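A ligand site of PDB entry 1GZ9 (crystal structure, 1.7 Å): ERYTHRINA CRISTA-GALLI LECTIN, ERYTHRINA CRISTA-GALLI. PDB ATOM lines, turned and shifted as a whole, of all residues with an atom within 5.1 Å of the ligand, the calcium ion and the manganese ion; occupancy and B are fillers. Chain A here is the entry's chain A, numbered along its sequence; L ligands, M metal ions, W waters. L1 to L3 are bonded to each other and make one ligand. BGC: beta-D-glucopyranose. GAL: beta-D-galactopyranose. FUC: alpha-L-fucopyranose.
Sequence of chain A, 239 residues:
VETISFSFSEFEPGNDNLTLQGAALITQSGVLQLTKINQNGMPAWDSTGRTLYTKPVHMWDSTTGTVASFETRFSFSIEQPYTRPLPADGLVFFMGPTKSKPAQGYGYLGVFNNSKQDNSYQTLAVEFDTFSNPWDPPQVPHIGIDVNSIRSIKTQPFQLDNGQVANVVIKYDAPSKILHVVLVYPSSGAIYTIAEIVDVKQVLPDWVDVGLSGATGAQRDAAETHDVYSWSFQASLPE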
ATOM      1  N   LEU A  86     -24.431   6.281  -9.123  1.00  0.00           N
ATOM      2  CA  LEU A  86     -23.907   5.102  -8.391  1.00  0.00           C
ATOM      3  C   LEU A  86     -25.102   4.313  -7.847  1.00  0.00           C
ATOM      4  O   LEU A  86     -26.098   4.895  -7.419  1.00  0.00           O
ATOM      5  CB  LEU A  86     -23.060   5.551  -7.208  1.00  0.00           C
ATOM      6  CG  LEU A  86     -21.715   6.199  -7.569  1.00  0.00           C
ATOM      7  CD1 LEU A  86     -21.023   6.645  -6.259  1.00  0.00           C
ATOM      8  CD2 LEU A  86     -20.836   5.236  -8.362  1.00  0.00           C
ATOM      9  N   ALA A  88     -27.372   1.929  -5.202  1.00  0.00           N
ATOM     10  CA  ALA A  88     -27.553   2.003  -3.731  1.00  0.00           C
ATOM     11  C   ALA A  88     -28.831   1.231  -3.423  1.00  0.00           C
ATOM     12  O   ALA A  88     -29.617   0.994  -4.344  1.00  0.00           O
ATOM     13  CB  ALA A  88     -27.706   3.454  -3.298  1.00  0.00           C
ATOM     14  N   ASP A  89     -29.064   0.792  -2.184  1.00  0.00           N
ATOM     15  CA  ASP A  89     -28.179   0.964  -1.024  1.00  0.00           C
ATOM     16  C   ASP A  89     -27.698  -0.394  -0.432  1.00  0.00           C
ATOM     17  O   ASP A  89     -26.637  -0.443   0.203  1.00  0.00           O
ATOM     18  CB  ASP A  89     -28.911   1.738   0.065  1.00  0.00           C
ATOM     19  CG  ASP A  89     -28.616   3.244   0.038  1.00  0.00           C
ATOM     20  OD1 ASP A  89     -27.490   3.655   0.420  1.00  0.00           O
ATOM     21  OD2 ASP A  89     -29.521   4.024  -0.371  1.00  0.00           O
ATOM     22  N   TYR A 106     -32.670   4.210   2.607  1.00  0.00           N
ATOM     23  CA  TYR A 106     -31.397   4.578   2.015  1.00  0.00           C
ATOM     24  C   TYR A 106     -30.275   3.810   2.696  1.00  0.00           C
ATOM     25  O   TYR A 106     -30.431   2.609   2.947  1.00  0.00           O
ATOM     26  CB  TYR A 106     -31.175   6.088   2.139  1.00  0.00           C
ATOM     27  CG  TYR A 106     -32.402   6.831   1.686  1.00  0.00           C
ATOM     28  CD1 TYR A 106     -33.016   6.514   0.470  1.00  0.00           C
ATOM     29  CD2 TYR A 106     -32.900   7.895   2.429  1.00  0.00           C
ATOM     30  CE1 TYR A 106     -34.097   7.256  -0.008  1.00  0.00           C
ATOM     31  CE2 TYR A 106     -33.996   8.655   1.956  1.00  0.00           C
ATOM     32  CZ  TYR A 106     -34.574   8.329   0.742  1.00  0.00           C
ATOM     33  OH  TYR A 106     -35.638   9.094   0.268  1.00  0.00           O
ATOM     34  N   GLY A 107     -29.190   4.504   3.031  1.00  0.00           N
ATOM     35  CA  GLY A 107     -28.042   3.847   3.635  1.00  0.00           C
ATOM     36  C   GLY A 107     -28.305   3.242   5.022  1.00  0.00           C
ATOM     37  O   GLY A 107     -27.450   2.500   5.552  1.00  0.00           O
ATOM     38  N   TYR A 108     -29.457   3.518   5.610  1.00  0.00           N
ATOM     39  CA  TYR A 108     -29.771   2.963   6.925  1.00  0.00           C
ATOM     40  C   TYR A 108     -30.436   1.597   6.805  1.00  0.00           C
ATOM     41  O   TYR A 108     -30.724   0.934   7.822  1.00  0.00           O
ATOM     42  CB  TYR A 108     -30.650   3.925   7.718  1.00  0.00           C
ATOM     43  CG  TYR A 108     -29.993   5.292   7.817  1.00  0.00           C
ATOM     44  CD1 TYR A 108     -28.926   5.518   8.678  1.00  0.00           C
ATOM     45  CD2 TYR A 108     -30.404   6.352   6.975  1.00  0.00           C
ATOM     46  CE1 TYR A 108     -28.269   6.755   8.718  1.00  0.00           C
ATOM     47  CE2 TYR A 108     -29.751   7.594   7.007  1.00  0.00           C
ATOM     48  CZ  TYR A 108     -28.687   7.775   7.882  1.00  0.00           C
ATOM     49  OH  TYR A 108     -28.000   8.975   7.874  1.00  0.00           O
ATOM     50  N   GLU A 127     -24.922  -6.942   6.899  1.00  0.00           N
ATOM     51  CA  GLU A 127     -25.257  -6.179   5.692  1.00  0.00           C
ATOM     52  C   GLU A 127     -24.437  -6.542   4.473  1.00  0.00           C
ATOM     53  O   GLU A 127     -23.339  -7.072   4.610  1.00  0.00           O
ATOM     54  CB  GLU A 127     -25.067  -4.698   5.991  1.00  0.00           C
ATOM     55  CG  GLU A 127     -23.609  -4.305   6.295  1.00  0.00           C
ATOM     56  CD  GLU A 127     -23.376  -2.798   6.350  1.00  0.00           C
ATOM     57  OE1 GLU A 127     -24.137  -2.057   7.047  1.00  0.00           O
ATOM     58  OE2 GLU A 127     -22.396  -2.404   5.696  1.00  0.00           O
ATOM     59  N   ASP A 129     -23.702  -4.240   1.636  1.00  0.00           N
ATOM     60  CA  ASP A 129     -23.844  -2.789   1.362  1.00  0.00           C
ATOM     61  C   ASP A 129     -23.237  -2.389   0.050  1.00  0.00           C
ATOM     62  O   ASP A 129     -22.061  -2.668  -0.202  1.00  0.00           O
ATOM     63  CB  ASP A 129     -23.145  -2.079   2.552  1.00  0.00           C
ATOM     64  CG  ASP A 129     -23.342  -0.570   2.576  1.00  0.00           C
ATOM     65  OD1 ASP A 129     -23.833  -0.013   1.595  1.00  0.00           O
ATOM     66  OD2 ASP A 129     -22.968   0.032   3.609  1.00  0.00           O
ATOM     67  N   PHE A 131     -23.411   0.980  -1.346  1.00  0.00           N
ATOM     68  CA  PHE A 131     -23.118   2.416  -1.548  1.00  0.00           C
ATOM     69  C   PHE A 131     -22.293   2.904  -0.395  1.00  0.00           C
ATOM     70  O   PHE A 131     -22.689   2.718   0.767  1.00  0.00           O
ATOM     71  CB  PHE A 131     -24.430   3.212  -1.604  1.00  0.00           C
ATOM     72  CG  PHE A 131     -24.207   4.719  -1.782  1.00  0.00           C
ATOM     73  CD1 PHE A 131     -24.141   5.281  -3.042  1.00  0.00           C
ATOM     74  CD2 PHE A 131     -24.036   5.533  -0.654  1.00  0.00           C
ATOM     75  CE1 PHE A 131     -23.895   6.671  -3.197  1.00  0.00           C
ATOM     76  CE2 PHE A 131     -23.785   6.918  -0.801  1.00  0.00           C
ATOM     77  CZ  PHE A 131     -23.710   7.483  -2.064  1.00  0.00           C
ATOM     78  N   SER A 132     -21.196   3.600  -0.691  1.00  0.00           N
ATOM     79  CA  SER A 132     -20.291   4.073   0.389  1.00  0.00           C
ATOM     80  C   SER A 132     -20.780   5.403   0.988  1.00  0.00           C
ATOM     81  O   SER A 132     -20.577   6.489   0.398  1.00  0.00           O
ATOM     82  CB  SER A 132     -18.868   4.271  -0.148  1.00  0.00           C
ATOM     83  OG  SER A 132     -17.961   4.517   0.916  1.00  0.00           O
ATOM     84  N   ASN A 133     -21.440   5.294   2.125  1.00  0.00           N
ATOM     85  CA  ASN A 133     -21.942   6.473   2.872  1.00  0.00           C
ATOM     86  C   ASN A 133     -20.770   7.101   3.676  1.00  0.00           C
ATOM     87  O   ASN A 133     -19.693   6.524   3.772  1.00  0.00           O
ATOM     88  CB  ASN A 133     -23.024   6.016   3.856  1.00  0.00           C
ATOM     89  CG  ASN A 133     -24.285   5.582   3.141  1.00  0.00           C
ATOM     90  OD1 ASN A 133     -24.459   4.407   2.790  1.00  0.00           O
ATOM     91  ND2 ASN A 133     -25.174   6.552   2.867  1.00  0.00           N
ATOM     92  N   PRO A 134     -20.995   8.256   4.306  1.00  0.00           N
ATOM     93  CA  PRO A 134     -19.930   8.912   5.081  1.00  0.00           C
ATOM     94  C   PRO A 134     -19.327   8.070   6.222  1.00  0.00           C
ATOM     95  O   PRO A 134     -18.194   8.357   6.670  1.00  0.00           O
ATOM     96  CB  PRO A 134     -20.630  10.185   5.617  1.00  0.00           C
ATOM     97  CG  PRO A 134     -21.634  10.497   4.510  1.00  0.00           C
ATOM     98  CD  PRO A 134     -22.193   9.114   4.189  1.00  0.00           C
ATOM     99  N   TRP A 135     -20.039   7.035   6.685  1.00  0.00           N
ATOM    100  CA  TRP A 135     -19.584   6.184   7.771  1.00  0.00           C
ATOM    101  C   TRP A 135     -19.048   4.837   7.264  1.00  0.00           C
ATOM    102  O   TRP A 135     -18.653   3.976   8.087  1.00  0.00           O
ATOM    103  CB  TRP A 135     -20.753   5.865   8.725  1.00  0.00           C
ATOM    104  CG  TRP A 135     -21.946   5.216   7.970  1.00  0.00           C
ATOM    105  CD1 TRP A 135     -22.071   3.890   7.585  1.00  0.00           C
ATOM    106  CD2 TRP A 135     -23.121   5.883   7.497  1.00  0.00           C
ATOM    107  NE1 TRP A 135     -23.260   3.699   6.893  1.00  0.00           N
ATOM    108  CE2 TRP A 135     -23.923   4.905   6.836  1.00  0.00           C
ATOM    109  CE3 TRP A 135     -23.585   7.212   7.569  1.00  0.00           C
ATOM    110  CZ2 TRP A 135     -25.156   5.231   6.254  1.00  0.00           C
ATOM    111  CZ3 TRP A 135     -24.803   7.528   6.987  1.00  0.00           C
ATOM    112  CH2 TRP A 135     -25.591   6.520   6.339  1.00  0.00           C
ATOM    113  N   ASP A 136     -19.059   4.658   5.944  1.00  0.00           N
ATOM    114  CA  ASP A 136     -18.626   3.388   5.332  1.00  0.00           C
ATOM    115  C   ASP A 136     -17.200   3.320   4.845  1.00  0.00           C
ATOM    116  O   ASP A 136     -16.570   4.332   4.612  1.00  0.00           O
ATOM    117  CB  ASP A 136     -19.443   3.106   4.038  1.00  0.00           C
ATOM    118  CG  ASP A 136     -20.818   2.497   4.311  1.00  0.00           C
ATOM    119  OD1 ASP A 136     -20.903   1.595   5.142  1.00  0.00           O
ATOM    120  OD2 ASP A 136     -21.796   2.926   3.669  1.00  0.00           O
ATOM    121  N   PRO A 137     -16.674   2.092   4.661  1.00  0.00           N
ATOM    122  CA  PRO A 137     -15.328   1.930   4.138  1.00  0.00           C
ATOM    123  C   PRO A 137     -15.560   2.293   2.680  1.00  0.00           C
ATOM    124  O   PRO A 137     -16.702   2.274   2.198  1.00  0.00           O
ATOM    125  CB  PRO A 137     -15.055   0.436   4.296  1.00  0.00           C
ATOM    126  CG  PRO A 137     -16.435  -0.174   4.320  1.00  0.00           C
ATOM    127  CD  PRO A 137     -17.187   0.808   5.184  1.00  0.00           C
ATOM    128  N   HIS A 142     -19.656  -4.285   0.158  1.00  0.00           N
ATOM    129  CA  HIS A 142     -18.940  -4.895   1.270  1.00  0.00           C
ATOM    130  C   HIS A 142     -19.930  -5.632   2.189  1.00  0.00           C
ATOM    131  O   HIS A 142     -21.122  -5.321   2.254  1.00  0.00           O
ATOM    132  CB  HIS A 142     -18.103  -3.860   2.095  1.00  0.00           C
ATOM    133  CG  HIS A 142     -18.891  -2.713   2.644  1.00  0.00           C
ATOM    134  ND1 HIS A 142     -18.923  -1.480   2.018  1.00  0.00           N
ATOM    135  CD2 HIS A 142     -19.648  -2.589   3.748  1.00  0.00           C
ATOM    136  CE1 HIS A 142     -19.680  -0.653   2.711  1.00  0.00           C
ATOM    137  NE2 HIS A 142     -20.137  -1.295   3.775  1.00  0.00           N
ATOM    138  N   ILE A 150     -25.268   1.370  12.239  1.00  0.00           N
ATOM    139  CA  ILE A 150     -25.077   1.160  10.799  1.00  0.00           C
ATOM    140  C   ILE A 150     -23.548   1.264  10.493  1.00  0.00           C
ATOM    141  O   ILE A 150     -23.081   0.896   9.402  1.00  0.00           O
ATOM    142  CB  ILE A 150     -25.833   2.250   9.973  1.00  0.00           C
ATOM    143  CG1 ILE A 150     -25.837   1.873   8.477  1.00  0.00           C
ATOM    144  CG2 ILE A 150     -25.178   3.602  10.153  1.00  0.00           C
ATOM    145  CD1 ILE A 150     -26.602   0.578   8.184  1.00  0.00           C
ATOM    146  N   SER A 152     -20.395  -0.309  10.760  1.00  0.00           N
ATOM    147  CA  SER A 152     -19.941  -1.670  11.063  1.00  0.00           C
ATOM    148  C   SER A 152     -18.718  -1.795  11.950  1.00  0.00           C
ATOM    149  O   SER A 152     -17.769  -1.022  11.784  1.00  0.00           O
ATOM    150  CB  SER A 152     -19.612  -2.400   9.765  1.00  0.00           C
ATOM    151  OG  SER A 152     -20.721  -2.374   8.891  1.00  0.00           O
ATOM    152  N   THR A 155     -15.820  -4.988   8.318  1.00  0.00           N
ATOM    153  CA  THR A 155     -16.337  -5.144   6.955  1.00  0.00           C
ATOM    154  C   THR A 155     -15.382  -5.956   6.107  1.00  0.00           C
ATOM    155  O   THR A 155     -14.199  -6.117   6.431  1.00  0.00           O
ATOM    156  CB  THR A 155     -16.578  -3.764   6.242  1.00  0.00           C
ATOM    157  OG1 THR A 155     -15.351  -3.020   6.219  1.00  0.00           O
ATOM    158  CG2 THR A 155     -17.612  -2.931   7.004  1.00  0.00           C
ATOM    159  N   THR A 216     -33.269   1.002  -1.734  1.00  0.00           N
ATOM    160  CA  THR A 216     -32.647   1.651  -2.891  1.00  0.00           C
ATOM    161  C   THR A 216     -32.446   3.095  -2.492  1.00  0.00           C
ATOM    162  O   THR A 216     -32.871   3.503  -1.399  1.00  0.00           O
ATOM    163  CB  THR A 216     -33.457   1.520  -4.217  1.00  0.00           C
ATOM    164  OG1 THR A 216     -34.803   1.930  -4.020  1.00  0.00           O
ATOM    165  CG2 THR A 216     -33.419   0.066  -4.668  1.00  0.00           C
ATOM    166  N   GLY A 217     -31.790   3.857  -3.366  1.00  0.00           N
ATOM    167  CA  GLY A 217     -31.347   5.205  -3.030  1.00  0.00           C
ATOM    168  C   GLY A 217     -32.196   6.447  -3.011  1.00  0.00           C
ATOM    169  O   GLY A 217     -33.347   6.414  -3.396  1.00  0.00           O
ATOM    170  N   ALA A 218     -31.561   7.544  -2.574  1.00  0.00           N
ATOM    171  CA  ALA A 218     -32.256   8.812  -2.394  1.00  0.00           C
ATOM    172  C   ALA A 218     -32.316   9.736  -3.577  1.00  0.00           C
ATOM    173  O   ALA A 218     -32.729  10.884  -3.432  1.00  0.00           O
ATOM    174  CB  ALA A 218     -31.679   9.558  -1.171  1.00  0.00           C
ATOM    175  N   GLN A 219     -31.898   9.270  -4.749  1.00  0.00           N
ATOM    176  CA  GLN A 219     -32.016  10.111  -5.924  1.00  0.00           C
ATOM    177  C   GLN A 219     -32.321   9.198  -7.089  1.00  0.00           C
ATOM    178  O   GLN A 219     -32.081   7.981  -7.023  1.00  0.00           O
ATOM    179  CB  GLN A 219     -30.740  10.930  -6.193  1.00  0.00           C
ATOM    180  CG  GLN A 219     -29.545  10.109  -6.617  1.00  0.00           C
ATOM    181  CD  GLN A 219     -28.340  10.988  -6.978  1.00  0.00           C
ATOM    182  OE1 GLN A 219     -27.978  11.096  -8.153  1.00  0.00           O
ATOM    183  NE2 GLN A 219     -27.725  11.593  -5.979  1.00  0.00           N
ATOM    184  N   ALA A 222     -30.555   5.652  -8.440  1.00  0.00           N
ATOM    185  CA  ALA A 222     -29.481   5.212  -7.515  1.00  0.00           C
ATOM    186  C   ALA A 222     -30.222   3.976  -6.999  1.00  0.00           C
ATOM    187  O   ALA A 222     -30.840   4.008  -5.929  1.00  0.00           O
ATOM    188  CB  ALA A 222     -29.281   6.249  -6.378  1.00  0.00           C
HETATM  189  C2  BGC L   1     -28.823  13.591  -2.811  1.00  0.00           C
HETATM  190  C3  BGC L   1     -29.075  12.204  -2.164  1.00  0.00           C
HETATM  191  C4  BGC L   1     -28.081  11.968  -1.010  1.00  0.00           C
HETATM  192  C5  BGC L   1     -28.134  13.107   0.024  1.00  0.00           C
HETATM  193  C6  BGC L   1     -27.008  13.013   1.052  1.00  0.00           C
HETATM  194  C1  BGC L   1     -28.950  14.654  -1.706  1.00  0.00           C
HETATM  195  O1  BGC L   1     -28.715  15.905  -2.270  1.00  0.00           O
HETATM  196  O2  BGC L   1     -29.795  13.785  -3.836  1.00  0.00           O
HETATM  197  O3  BGC L   1     -28.959  11.214  -3.160  1.00  0.00           O
HETATM  198  O4  BGC L   1     -28.429  10.722  -0.248  1.00  0.00           O
HETATM  199  O5  BGC L   1     -27.939  14.385  -0.667  1.00  0.00           O
HETATM  200  O6  BGC L   1     -27.381  13.713   2.255  1.00  0.00           O
HETATM  201  C1  GAL L   2     -27.659   9.504  -0.515  1.00  0.00           C
HETATM  202  C2  GAL L   2     -28.022   8.572   0.579  1.00  0.00           C
HETATM  203  C3  GAL L   2     -27.191   7.230   0.238  1.00  0.00           C
HETATM  204  C4  GAL L   2     -27.619   6.710  -1.148  1.00  0.00           C
HETATM  205  C5  GAL L   2     -27.293   7.837  -2.163  1.00  0.00           C
HETATM  206  C6  GAL L   2     -27.682   7.493  -3.558  1.00  0.00           C
HETATM  207  O2  GAL L   2     -27.534   9.192   1.776  1.00  0.00           O
HETATM  208  O3  GAL L   2     -27.504   6.241   1.262  1.00  0.00           O
HETATM  209  O4  GAL L   2     -29.021   6.442  -1.222  1.00  0.00           O
HETATM  210  O5  GAL L   2     -28.026   9.028  -1.806  1.00  0.00           O
HETATM  211  O6  GAL L   2     -27.200   8.569  -4.382  1.00  0.00           O
HETATM  212  C1  FUC L   3     -27.847   8.769   3.089  1.00  0.00           C
HETATM  213  C2  FUC L   3     -26.832   9.524   3.982  1.00  0.00           C
HETATM  214  C3  FUC L   3     -27.064  11.058   4.188  1.00  0.00           C
HETATM  215  C4  FUC L   3     -28.579  11.366   4.440  1.00  0.00           C
HETATM  216  C5  FUC L   3     -29.446  10.707   3.325  1.00  0.00           C
HETATM  217  C6  FUC L   3     -30.994  10.969   3.531  1.00  0.00           C
HETATM  218  O2  FUC L   3     -25.480   9.052   3.772  1.00  0.00           O
HETATM  219  O3  FUC L   3     -26.300  11.471   5.317  1.00  0.00           O
HETATM  220  O4  FUC L   3     -28.967  10.848   5.700  1.00  0.00           O
HETATM  221  O5  FUC L   3     -29.249   9.190   3.296  1.00  0.00           O
HETATM  222 CA    CA M   1     -23.846   2.115   2.758  1.00  0.00          CA
HETATM  223 MN    MN M   2     -21.636  -0.387   5.278  1.00  0.00          MN
HETATM  224  O   HOH W   1     -24.469  10.417   1.588  1.00  0.00           O
HETATM  225  O   HOH W   2     -30.033  14.717   2.820  1.00  0.00           O
HETATM  226  O   HOH W   3     -26.071   7.598  -6.471  1.00  0.00           O
HETATM  227  O   HOH W   4     -32.777  13.430  -4.484  1.00  0.00           O
HETATM  228  O   HOH W   5     -24.783  15.592   0.416  1.00  0.00           O
HETATM  229  O   HOH W   6     -31.153  11.689   6.889  1.00  0.00           O
HETATM  230  O   HOH W   7     -23.324   0.354   6.709  1.00  0.00           O
HETATM  231  O   HOH W   8     -24.832   1.820   4.935  1.00  0.00           O
HETATM  232  O   HOH W   9     -25.861   1.922   1.522  1.00  0.00           O
HETATM  233  O   HOH W  10     -20.208  -0.549   6.954  1.00  0.00           O
HETATM  234  O   HOH W  11     -25.236  10.525  -3.505  1.00  0.00           O
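NE2 of Gln 219 is in hydrogen-bond range of O3 of BGC L1, at 3.1 Å.
An oxygen (O4) of GAL L2 lies within hydrogen-bond range of the backbone NH of Ala 218, at 3.1 Å.
An oxygen (O4) of FUC L3 sits at hydrogen-bond distance from the side-chain hydroxyl (OH) of Tyr 108 (3.0 Å).
The side-chain carboxylate of Asp 89 lies within hydrogen-bond range of an oxygen (O4) of GAL L2, at 2.6 Å.
An oxygen (O2) of FUC L3 is in hydrogen-bond range of the side-chain amide nitrogen of Asn 133, 2.7 Å away.
N of Gly 107 is in hydrogen-bond range of O3 of GAL L2, 3.0 Å away.
N of Gly 217 is in hydrogen-bond range of O of Ala 222, 2.7 Å away.
The side-chain carboxylate (OD1) of Asp 89 lies within hydrogen-bond range of the backbone NH (N) of Gly 107, 3.2 Å away.
Merely in contact with the ligand: Gly 217, Pro 134, Ala 222, Trp 135, Tyr 106 and Ala 88.
Of the 24 residues printed, 13 come within 4 Å of the ligand.
Within 4 Å of the calcium ion: Asp 129, Phe 131, Asn 133 and Asp 136.
Four residues have an atom within 4 Å of the manganese ion: Glu 127, Asp 129, Asp 136 and His 142.
The nearest printed residue that does not touch the manganese ion is Ser 152 (4.2 Å).
The calcium ion is bound by water W9 (2.4 Å).
The side-chain amide oxygen (OD1) of Asn 133 binds the calcium ion, 2.4 Å away.
The backbone carbonyl oxygen (O) of Phe 131 binds the calcium ion (2.4 Å).
The calcium ion is bound by OD2 of Asp 136, at 2.4 Å.
Water W8 binds the calcium ion, at 2.4 Å.
The calcium ion is bound by the side-chain carboxylate (OD2) of Asp 129, 2.4 Å away.
OD1 of Asp 129 binds the calcium ion, 2.4 Å away.
The calcium ion has seven donor atoms within binding distance.
The manganese ion is bound by the side-chain carboxylate (OD1) of Asp 136, the side-chain carboxylate (OD2) of Asp 129, the side-chain carboxylate (OE2) of Glu 127, water W10, a ring nitrogen (NE2) of His 142 and water W7.
The manganese ion has six donor atoms within binding distance.
Water W8 lies within hydrogen-bond range of O of Gly 107 and NE1 of Trp 135.
Water W7 lies within hydrogen-bond range of the side-chain carboxylate (OE1) of Glu 127 (2.6 Å), the backbone carbonyl oxygen (O) of Ile 150 (2.8 Å) and the indole nitrogen (NE1) of Trp 135 (3.4 Å).
Water W3 bridges an oxygen (O6) of GAL L2 and the backbone carbonyl oxygen of Leu 86.
Water W4 lies within hydrogen-bond range of the backbone carbonyl oxygen (O) of Ala 218 (2.8 Å) and an oxygen (O2) of BGC L1 (3.1 Å).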
